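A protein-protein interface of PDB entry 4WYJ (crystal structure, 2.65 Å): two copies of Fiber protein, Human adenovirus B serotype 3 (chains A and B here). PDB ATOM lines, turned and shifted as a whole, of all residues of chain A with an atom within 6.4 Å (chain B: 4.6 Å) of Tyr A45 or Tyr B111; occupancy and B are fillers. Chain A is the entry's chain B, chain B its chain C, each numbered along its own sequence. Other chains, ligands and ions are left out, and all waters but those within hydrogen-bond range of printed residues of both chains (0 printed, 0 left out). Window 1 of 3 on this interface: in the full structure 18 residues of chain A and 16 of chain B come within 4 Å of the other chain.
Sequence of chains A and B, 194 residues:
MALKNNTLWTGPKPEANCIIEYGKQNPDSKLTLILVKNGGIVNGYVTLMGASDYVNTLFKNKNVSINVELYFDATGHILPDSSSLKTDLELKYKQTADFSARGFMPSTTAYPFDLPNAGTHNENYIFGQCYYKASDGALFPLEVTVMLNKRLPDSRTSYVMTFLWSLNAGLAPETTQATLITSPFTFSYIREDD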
ATOM      1  N   PRO A  12      21.964  22.703 -14.219  1.00  0.00           N
ATOM      2  CA  PRO A  12      20.749  21.871 -14.424  1.00  0.00           C
ATOM      3  C   PRO A  12      20.156  21.194 -13.191  1.00  0.00           C
ATOM      4  O   PRO A  12      18.991  20.816 -13.232  1.00  0.00           O
ATOM      5  CB  PRO A  12      21.225  20.791 -15.418  1.00  0.00           C
ATOM      6  CG  PRO A  12      22.687  20.718 -15.207  1.00  0.00           C
ATOM      7  CD  PRO A  12      23.160  22.090 -14.839  1.00  0.00           C
ATOM      8  N   LYS A  13      20.968  20.956 -12.148  1.00  0.00           N
ATOM      9  CA  LYS A  13      20.586  20.224 -10.943  1.00  0.00           C
ATOM     10  C   LYS A  13      21.447  20.765  -9.796  1.00  0.00           C
ATOM     11  O   LYS A  13      22.442  20.139  -9.408  1.00  0.00           O
ATOM     12  CB  LYS A  13      20.847  18.720 -11.198  1.00  0.00           C
ATOM     13  CG  LYS A  13      20.026  17.770 -10.372  1.00  0.00           C
ATOM     14  CD  LYS A  13      18.515  17.907 -10.618  1.00  0.00           C
ATOM     15  CE  LYS A  13      17.849  16.554 -10.577  1.00  0.00           C
ATOM     16  NZ  LYS A  13      16.697  16.567  -9.670  1.00  0.00           N
ATOM     17  N   THR A  32      16.348  26.029  -9.194  1.00  0.00           N
ATOM     18  CA  THR A  32      16.791  25.901 -10.573  1.00  0.00           C
ATOM     19  C   THR A  32      16.154  27.077 -11.320  1.00  0.00           C
ATOM     20  O   THR A  32      14.929  27.172 -11.400  1.00  0.00           O
ATOM     21  CB  THR A  32      16.402  24.557 -11.205  1.00  0.00           C
ATOM     22  OG1 THR A  32      16.953  23.489 -10.429  1.00  0.00           O
ATOM     23  CG2 THR A  32      16.883  24.436 -12.655  1.00  0.00           C
ATOM     24  N   LEU A  33      16.988  28.001 -11.787  1.00  0.00           N
ATOM     25  CA  LEU A  33      16.572  29.169 -12.555  1.00  0.00           C
ATOM     26  C   LEU A  33      17.412  29.220 -13.834  1.00  0.00           C
ATOM     27  O   LEU A  33      18.639  29.169 -13.758  1.00  0.00           O
ATOM     28  CB  LEU A  33      16.698  30.479 -11.739  1.00  0.00           C
ATOM     29  CG  LEU A  33      16.220  31.765 -12.463  1.00  0.00           C
ATOM     30  CD1 LEU A  33      14.687  31.756 -12.743  1.00  0.00           C
ATOM     31  CD2 LEU A  33      16.590  32.971 -11.687  1.00  0.00           C
ATOM     32  N   ILE A  34      16.729  29.249 -15.003  1.00  0.00           N
ATOM     33  CA  ILE A  34      17.348  29.306 -16.330  1.00  0.00           C
ATOM     34  C   ILE A  34      16.763  30.497 -17.090  1.00  0.00           C
ATOM     35  O   ILE A  34      15.541  30.605 -17.240  1.00  0.00           O
ATOM     36  CB  ILE A  34      17.196  27.988 -17.114  1.00  0.00           C
ATOM     37  CG1 ILE A  34      17.668  26.776 -16.273  1.00  0.00           C
ATOM     38  CG2 ILE A  34      17.921  28.063 -18.466  1.00  0.00           C
ATOM     39  CD1 ILE A  34      17.297  25.474 -16.839  1.00  0.00           C
ATOM     40  N   LEU A  35      17.633  31.414 -17.521  1.00  0.00           N
ATOM     41  CA  LEU A  35      17.255  32.609 -18.276  1.00  0.00           C
ATOM     42  C   LEU A  35      17.915  32.532 -19.650  1.00  0.00           C
ATOM     43  O   LEU A  35      19.153  32.556 -19.765  1.00  0.00           O
ATOM     44  CB  LEU A  35      17.663  33.906 -17.520  1.00  0.00           C
ATOM     45  CG  LEU A  35      17.072  34.097 -16.110  1.00  0.00           C
ATOM     46  CD1 LEU A  35      17.734  35.264 -15.396  1.00  0.00           C
ATOM     47  CD2 LEU A  35      15.524  34.237 -16.147  1.00  0.00           C
ATOM     48  N   VAL A  36      17.085  32.382 -20.691  1.00  0.00           N
ATOM     49  CA  VAL A  36      17.597  32.266 -22.061  1.00  0.00           C
ATOM     50  C   VAL A  36      17.220  33.507 -22.885  1.00  0.00           C
ATOM     51  O   VAL A  36      16.049  33.862 -22.938  1.00  0.00           O
ATOM     52  CB  VAL A  36      17.176  30.932 -22.755  1.00  0.00           C
ATOM     53  CG1 VAL A  36      17.841  30.783 -24.122  1.00  0.00           C
ATOM     54  CG2 VAL A  36      17.472  29.718 -21.871  1.00  0.00           C
ATOM     55  N   ASN A  43      13.407  33.940 -22.118  1.00  0.00           N
ATOM     56  CA  ASN A  43      12.576  32.767 -21.818  1.00  0.00           C
ATOM     57  C   ASN A  43      13.088  32.168 -20.479  1.00  0.00           C
ATOM     58  O   ASN A  43      14.234  31.724 -20.374  1.00  0.00           O
ATOM     59  CB  ASN A  43      12.615  31.738 -22.952  1.00  0.00           C
ATOM     60  CG  ASN A  43      11.922  32.174 -24.217  1.00  0.00           C
ATOM     61  OD1 ASN A  43      10.823  32.731 -24.203  1.00  0.00           O
ATOM     62  ND2 ASN A  43      12.534  31.885 -25.351  1.00  0.00           N
ATOM     63  N   GLY A  44      12.258  32.260 -19.460  1.00  0.00           N
ATOM     64  CA  GLY A  44      12.594  31.806 -18.119  1.00  0.00           C
ATOM     65  C   GLY A  44      11.986  30.469 -17.764  1.00  0.00           C
ATOM     66  O   GLY A  44      10.912  30.111 -18.267  1.00  0.00           O
ATOM     67  N   TYR A  45      12.699  29.721 -16.899  1.00  0.00           N
ATOM     68  CA  TYR A  45      12.354  28.379 -16.411  1.00  0.00           C
ATOM     69  C   TYR A  45      12.744  28.329 -14.924  1.00  0.00           C
ATOM     70  O   TYR A  45      13.904  28.581 -14.575  1.00  0.00           O
ATOM     71  CB  TYR A  45      13.115  27.309 -17.233  1.00  0.00           C
ATOM     72  CG  TYR A  45      12.984  25.878 -16.759  1.00  0.00           C
ATOM     73  CD1 TYR A  45      13.742  25.404 -15.690  1.00  0.00           C
ATOM     74  CD2 TYR A  45      12.166  24.970 -17.434  1.00  0.00           C
ATOM     75  CE1 TYR A  45      13.656  24.076 -15.270  1.00  0.00           C
ATOM     76  CE2 TYR A  45      12.077  23.637 -17.029  1.00  0.00           C
ATOM     77  CZ  TYR A  45      12.838  23.189 -15.951  1.00  0.00           C
ATOM     78  OH  TYR A  45      12.797  21.884 -15.519  1.00  0.00           O
ATOM     79  N   VAL A  46      11.771  28.038 -14.052  1.00  0.00           N
ATOM     80  CA  VAL A  46      12.028  28.007 -12.620  1.00  0.00           C
ATOM     81  C   VAL A  46      11.337  26.814 -11.945  1.00  0.00           C
ATOM     82  O   VAL A  46      10.179  26.468 -12.240  1.00  0.00           O
ATOM     83  CB  VAL A  46      11.727  29.366 -11.915  1.00  0.00           C
ATOM     84  CG1 VAL A  46      10.228  29.684 -11.870  1.00  0.00           C
ATOM     85  CG2 VAL A  46      12.354  29.439 -10.522  1.00  0.00           C
ATOM     86  N   THR A  47      12.098  26.179 -11.041  1.00  0.00           N
ATOM     87  CA  THR A  47      11.638  25.054 -10.239  1.00  0.00           C
ATOM     88  C   THR A  47      12.302  25.156  -8.859  1.00  0.00           C
ATOM     89  O   THR A  47      13.424  25.653  -8.765  1.00  0.00           O
ATOM     90  CB  THR A  47      11.797  23.702 -11.002  1.00  0.00           C
ATOM     91  OG1 THR A  47      11.164  22.673 -10.256  1.00  0.00           O
ATOM     92  CG2 THR A  47      13.227  23.299 -11.216  1.00  0.00           C
ATOM     93  N   PRO A 184       7.942  22.466 -13.201  1.00  0.00           N
ATOM     94  CA  PRO A 184       8.522  23.606 -13.937  1.00  0.00           C
ATOM     95  C   PRO A 184       7.513  24.668 -14.363  1.00  0.00           C
ATOM     96  O   PRO A 184       6.454  24.339 -14.888  1.00  0.00           O
ATOM     97  CB  PRO A 184       9.193  22.933 -15.143  1.00  0.00           C
ATOM     98  CG  PRO A 184       9.483  21.573 -14.701  1.00  0.00           C
ATOM     99  CD  PRO A 184       8.296  21.191 -13.866  1.00  0.00           C
ATOM    100  N   PHE A 185       7.821  25.924 -14.049  1.00  0.00           N
ATOM    101  CA  PHE A 185       7.059  27.133 -14.381  1.00  0.00           C
ATOM    102  C   PHE A 185       7.916  27.922 -15.380  1.00  0.00           C
ATOM    103  O   PHE A 185       9.101  28.185 -15.132  1.00  0.00           O
ATOM    104  CB  PHE A 185       6.732  27.976 -13.129  1.00  0.00           C
ATOM    105  CG  PHE A 185       6.022  29.282 -13.424  1.00  0.00           C
ATOM    106  CD1 PHE A 185       4.672  29.300 -13.743  1.00  0.00           C
ATOM    107  CD2 PHE A 185       6.716  30.492 -13.417  1.00  0.00           C
ATOM    108  CE1 PHE A 185       4.025  30.500 -14.077  1.00  0.00           C
ATOM    109  CE2 PHE A 185       6.076  31.695 -13.738  1.00  0.00           C
ATOM    110  CZ  PHE A 185       4.727  31.693 -14.065  1.00  0.00           C
ATOM    111  N   THR A 186       7.316  28.246 -16.526  1.00  0.00           N
ATOM    112  CA  THR A 186       7.934  28.989 -17.617  1.00  0.00           C
ATOM    113  C   THR A 186       7.210  30.322 -17.779  1.00  0.00           C
ATOM    114  O   THR A 186       5.985  30.393 -17.622  1.00  0.00           O
ATOM    115  CB  THR A 186       7.940  28.185 -18.915  1.00  0.00           C
ATOM    116  OG1 THR A 186       6.593  27.897 -19.299  1.00  0.00           O
ATOM    117  CG2 THR A 186       8.749  26.922 -18.810  1.00  0.00           C
ATOM    118  N   PHE A 187       7.972  31.368 -18.102  1.00  0.00           N
ATOM    119  CA  PHE A 187       7.504  32.745 -18.259  1.00  0.00           C
ATOM    120  C   PHE A 187       8.466  33.480 -19.201  1.00  0.00           C
ATOM    121  O   PHE A 187       9.590  33.006 -19.425  1.00  0.00           O
ATOM    122  CB  PHE A 187       7.455  33.448 -16.882  1.00  0.00           C
ATOM    123  CG  PHE A 187       8.787  33.505 -16.152  1.00  0.00           C
ATOM    124  CD1 PHE A 187       9.291  32.381 -15.494  1.00  0.00           C
ATOM    125  CD2 PHE A 187       9.538  34.679 -16.131  1.00  0.00           C
ATOM    126  CE1 PHE A 187      10.524  32.425 -14.850  1.00  0.00           C
ATOM    127  CE2 PHE A 187      10.762  34.727 -15.477  1.00  0.00           C
ATOM    128  CZ  PHE A 187      11.245  33.602 -14.833  1.00  0.00           C
ATOM    129  N   PRO B 106      15.653  15.108 -23.374  1.00  0.00           N
ATOM    130  CA  PRO B 106      15.612  15.610 -21.980  1.00  0.00           C
ATOM    131  C   PRO B 106      16.871  15.176 -21.201  1.00  0.00           C
ATOM    132  O   PRO B 106      17.274  14.012 -21.287  1.00  0.00           O
ATOM    133  CB  PRO B 106      14.330  14.992 -21.418  1.00  0.00           C
ATOM    134  CG  PRO B 106      14.118  13.744 -22.249  1.00  0.00           C
ATOM    135  CD  PRO B 106      14.631  14.059 -23.611  1.00  0.00           C
ATOM    136  N   SER B 107      17.515  16.128 -20.480  1.00  0.00           N
ATOM    137  CA  SER B 107      18.726  15.900 -19.681  1.00  0.00           C
ATOM    138  C   SER B 107      18.523  14.795 -18.661  1.00  0.00           C
ATOM    139  O   SER B 107      17.545  14.828 -17.917  1.00  0.00           O
ATOM    140  CB  SER B 107      19.145  17.179 -18.955  1.00  0.00           C
ATOM    141  OG  SER B 107      20.170  16.937 -18.002  1.00  0.00           O
ATOM    142  N   THR B 108      19.453  13.827 -18.615  1.00  0.00           N
ATOM    143  CA  THR B 108      19.398  12.739 -17.631  1.00  0.00           C
ATOM    144  C   THR B 108      19.993  13.234 -16.308  1.00  0.00           C
ATOM    145  O   THR B 108      19.922  12.532 -15.298  1.00  0.00           O
ATOM    146  CB  THR B 108      20.044  11.453 -18.148  1.00  0.00           C
ATOM    147  OG1 THR B 108      21.316  11.775 -18.678  1.00  0.00           O
ATOM    148  CG2 THR B 108      19.211  10.749 -19.211  1.00  0.00           C
ATOM    149  N   THR B 109      20.564  14.450 -16.310  1.00  0.00           N
ATOM    150  CA  THR B 109      21.098  15.065 -15.105  1.00  0.00           C
ATOM    151  C   THR B 109      19.923  15.714 -14.375  1.00  0.00           C
ATOM    152  O   THR B 109      19.714  15.441 -13.191  1.00  0.00           O
ATOM    153  CB  THR B 109      22.269  16.018 -15.413  1.00  0.00           C
ATOM    154  OG1 THR B 109      23.302  15.284 -16.106  1.00  0.00           O
ATOM    155  CG2 THR B 109      22.860  16.652 -14.129  1.00  0.00           C
ATOM    156  N   ALA B 110      19.135  16.533 -15.092  1.00  0.00           N
ATOM    157  CA  ALA B 110      17.974  17.224 -14.544  1.00  0.00           C
ATOM    158  C   ALA B 110      16.809  16.253 -14.288  1.00  0.00           C
ATOM    159  O   ALA B 110      16.116  16.360 -13.261  1.00  0.00           O
ATOM    160  CB  ALA B 110      17.534  18.327 -15.491  1.00  0.00           C
ATOM    161  N   TYR B 111      16.596  15.305 -15.231  1.00  0.00           N
ATOM    162  CA  TYR B 111      15.523  14.304 -15.201  1.00  0.00           C
ATOM    163  C   TYR B 111      16.148  12.895 -15.209  1.00  0.00           C
ATOM    164  O   TYR B 111      16.285  12.263 -16.274  1.00  0.00           O
ATOM    165  CB  TYR B 111      14.550  14.538 -16.382  1.00  0.00           C
ATOM    166  CG  TYR B 111      14.286  16.008 -16.655  1.00  0.00           C
ATOM    167  CD1 TYR B 111      13.561  16.790 -15.753  1.00  0.00           C
ATOM    168  CD2 TYR B 111      14.822  16.636 -17.777  1.00  0.00           C
ATOM    169  CE1 TYR B 111      13.352  18.149 -15.980  1.00  0.00           C
ATOM    170  CE2 TYR B 111      14.631  17.998 -18.004  1.00  0.00           C
ATOM    171  CZ  TYR B 111      13.876  18.743 -17.116  1.00  0.00           C
ATOM    172  OH  TYR B 111      13.645  20.067 -17.371  1.00  0.00           O
ATOM    173  N   PRO B 112      16.646  12.431 -14.025  1.00  0.00           N
ATOM    174  CA  PRO B 112      17.299  11.117 -13.971  1.00  0.00           C
ATOM    175  C   PRO B 112      16.303   9.968 -14.054  1.00  0.00           C
ATOM    176  O   PRO B 112      15.096  10.169 -14.132  1.00  0.00           O
ATOM    177  CB  PRO B 112      18.006  11.131 -12.608  1.00  0.00           C
ATOM    178  CG  PRO B 112      17.856  12.487 -12.067  1.00  0.00           C
ATOM    179  CD  PRO B 112      16.631  13.052 -12.685  1.00  0.00           C
ATOM    180  N   PHE B 113      16.835   8.749 -14.044  1.00  0.00           N
ATOM    181  CA  PHE B 113      16.072   7.515 -14.045  1.00  0.00           C
ATOM    182  C   PHE B 113      15.993   7.030 -12.608  1.00  0.00           C
ATOM    183  O   PHE B 113      17.021   7.035 -11.914  1.00  0.00           O
ATOM    184  CB  PHE B 113      16.749   6.470 -14.944  1.00  0.00           C
ATOM    185  CG  PHE B 113      16.509   6.784 -16.399  1.00  0.00           C
ATOM    186  CD1 PHE B 113      15.286   6.500 -16.997  1.00  0.00           C
ATOM    187  CD2 PHE B 113      17.485   7.416 -17.162  1.00  0.00           C
ATOM    188  CE1 PHE B 113      15.051   6.827 -18.333  1.00  0.00           C
ATOM    189  CE2 PHE B 113      17.241   7.757 -18.495  1.00  0.00           C
ATOM    190  CZ  PHE B 113      16.029   7.447 -19.076  1.00  0.00           C
ATOM    191  N   GLU B 123      10.588  15.377 -10.047  1.00  0.00           N
ATOM    192  CA  GLU B 123      11.057  16.577 -10.731  1.00  0.00           C
ATOM    193  C   GLU B 123      11.024  16.380 -12.238  1.00  0.00           C
ATOM    194  O   GLU B 123      11.341  17.319 -12.968  1.00  0.00           O
ATOM    195  CB  GLU B 123      12.479  16.952 -10.275  1.00  0.00           C
ATOM    196  CG  GLU B 123      13.536  15.883 -10.500  1.00  0.00           C
ATOM    197  CD  GLU B 123      13.823  15.010  -9.299  1.00  0.00           C
ATOM    198  OE1 GLU B 123      12.897  14.785  -8.488  1.00  0.00           O
ATOM    199  OE2 GLU B 123      14.978  14.547  -9.164  1.00  0.00           O
ATOM    200  N   ASN B 124      10.666  15.158 -12.694  1.00  0.00           N
ATOM    201  CA  ASN B 124      10.617  14.715 -14.090  1.00  0.00           C
ATOM    202  C   ASN B 124       9.286  14.964 -14.755  1.00  0.00           C
ATOM    203  O   ASN B 124       9.126  14.646 -15.951  1.00  0.00           O
ATOM    204  CB  ASN B 124      10.941  13.222 -14.178  1.00  0.00           C
ATOM    205  CG  ASN B 124      12.375  12.882 -13.912  1.00  0.00           C
ATOM    206  OD1 ASN B 124      13.046  13.540 -13.111  1.00  0.00           O
ATOM    207  ND2 ASN B 124      12.849  11.784 -14.506  1.00  0.00           N
ATOM    208  N   LEU B 148       9.390  13.018 -18.315  1.00  0.00           N
ATOM    209  CA  LEU B 148      10.693  12.965 -18.989  1.00  0.00           C
ATOM    210  C   LEU B 148      11.522  11.939 -18.266  1.00  0.00           C
ATOM    211  O   LEU B 148      11.582  11.959 -17.029  1.00  0.00           O
ATOM    212  CB  LEU B 148      11.399  14.339 -18.989  1.00  0.00           C
ATOM    213  CG  LEU B 148      10.574  15.536 -19.500  1.00  0.00           C
ATOM    214  CD1 LEU B 148      11.215  16.847 -19.063  1.00  0.00           C
ATOM    215  CD2 LEU B 148      10.334  15.457 -21.040  1.00  0.00           C
ATOM    216  N   ASN B 149      12.088  10.991 -19.029  1.00  0.00           N
ATOM    217  CA  ASN B 149      12.962   9.928 -18.527  1.00  0.00           C
ATOM    218  C   ASN B 149      12.266   9.134 -17.390  1.00  0.00           C
ATOM    219  O   ASN B 149      11.218   8.544 -17.677  1.00  0.00           O
ATOM    220  CB  ASN B 149      14.342  10.516 -18.171  1.00  0.00           C
ATOM    221  CG  ASN B 149      15.048  11.115 -19.387  1.00  0.00           C
ATOM    222  OD1 ASN B 149      14.783  10.755 -20.533  1.00  0.00           O
ATOM    223  ND2 ASN B 149      15.953  12.055 -19.184  1.00  0.00           N
ATOM    224  N   SER B 188       8.727  23.536 -21.705  1.00  0.00           N
ATOM    225  CA  SER B 188      10.177  23.683 -21.824  1.00  0.00           C
ATOM    226  C   SER B 188      10.889  22.713 -20.870  1.00  0.00           C
ATOM    227  O   SER B 188      10.430  22.467 -19.750  1.00  0.00           O
ATOM    228  CB  SER B 188      10.598  25.111 -21.471  1.00  0.00           C
ATOM    229  OG  SER B 188      10.167  26.079 -22.408  1.00  0.00           O
ATOM    230  N   TYR B 189      12.029  22.204 -21.289  1.00  0.00           N
ATOM    231  CA  TYR B 189      12.813  21.327 -20.438  1.00  0.00           C
ATOM    232  C   TYR B 189      14.302  21.554 -20.670  1.00  0.00           C
ATOM    233  O   TYR B 189      14.695  22.010 -21.750  1.00  0.00           O
ATOM    234  CB  TYR B 189      12.416  19.834 -20.630  1.00  0.00           C
ATOM    235  CG  TYR B 189      12.547  19.302 -22.041  1.00  0.00           C
ATOM    236  CD1 TYR B 189      11.477  19.347 -22.926  1.00  0.00           C
ATOM    237  CD2 TYR B 189      13.727  18.710 -22.478  1.00  0.00           C
ATOM    238  CE1 TYR B 189      11.574  18.818 -24.211  1.00  0.00           C
ATOM    239  CE2 TYR B 189      13.852  18.211 -23.773  1.00  0.00           C
ATOM    240  CZ  TYR B 189      12.771  18.257 -24.632  1.00  0.00           C
ATOM    241  OH  TYR B 189      12.898  17.760 -25.904  1.00  0.00           O
ATOM    242  N   ILE B 190      15.125  21.212 -19.664  1.00  0.00           N
ATOM    243  CA  ILE B 190      16.585  21.276 -19.741  1.00  0.00           C
ATOM    244  C   ILE B 190      17.029  20.159 -20.718  1.00  0.00           C
ATOM    245  O   ILE B 190      16.710  18.987 -20.502  1.00  0.00           O
ATOM    246  CB  ILE B 190      17.198  21.117 -18.321  1.00  0.00           C
ATOM    247  CG1 ILE B 190      16.618  22.189 -17.355  1.00  0.00           C
ATOM    248  CG2 ILE B 190      18.731  21.149 -18.369  1.00  0.00           C
ATOM    249  CD1 ILE B 190      16.821  21.983 -15.857  1.00  0.00           C
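The side-chain carboxylate (OE2) of Glu B123 is in salt-bridge range of the side-chain amino group (NZ) of Lys A13, at 2.7 Å.
The side-chain hydroxyl of Tyr A45 sits at hydrogen-bond distance from the side-chain hydroxyl of Tyr B111 (2.7 Å).
The backbone carbonyl oxygen of Tyr A45 sits at hydrogen-bond distance from the backbone NH of Ile A34, at 2.9 Å.
The side-chain hydroxyl (OG) of Ser B107 lies within hydrogen-bond range of the backbone NH (N) of Thr B109 (3.0 Å).
OG of Ser B107 is in hydrogen-bond range of N of Ala B110 (3.1 Å).
The backbone NH (N) of Ser B107 sits at hydrogen-bond distance from the backbone carbonyl oxygen (O) of Ile B190 (3.0 Å).
ND2 of Asn B149 sits at hydrogen-bond distance from O of Tyr B111 (2.9 Å).
The side-chain hydroxyl (OH) of Tyr B111 lies within hydrogen-bond range of the backbone NH (N) of Ile B190 (3.0 Å).
Pro A12 touches Ala B110.
O of Pro A12 touches CD1 of Ile B190, 3.6 Å away.
O of Thr B109 touches CE of Lys A13 (3.4 Å).
Lys A13 touches Ala B110 (CE to O, 3.2 Å).
CD1 of Ile A34 touches CG1 of Ile B190, at 3.4 Å.
Ser B188 touches Tyr A45.
CE1 of Tyr A45 touches CD1 of Ile B190 (3.8 Å).
CG2 of Thr A186 touches CB of Ser B188, 3.7 Å away.
Of chain B, only Tyr B111 (2.7 Å), Ser B188 (3.4 Å) and Ile B190 (3.8 Å) come within 4 Å of Tyr A45.
Tyr B111 touches just one residue of chain A: Tyr A45.
Printed residues of chain A within 4 Å of Ala B110: Pro A12 (3.7 Å) and Lys A13 (3.2 Å).
Of the printed residues of chain B, Pro A12 touches Ala B110 (3.7 Å) and Ile B190 (3.6 Å).
Of the printed residues of chain A, Ser B188 touches Tyr A45 (3.4 Å) and Thr A186 (3.7 Å).
Of the printed residues of chain B, Thr A186 touches Ser B188 (3.7 Å).
The nearest residue of chain A that does not touch Tyr B111 is Lys A13 (5.0 Å).
The nearest printed residue of chain B that does not touch Lys A13 is Pro B112 (4.3 Å).
Along chain B the printed residues that touch a printed residue of chain A span positions 109 to 190.
No position is printed for both chains.
Of the 10 pairs that touch across the chains among the printed residues, none has its exchanged pair printed and touching as well.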
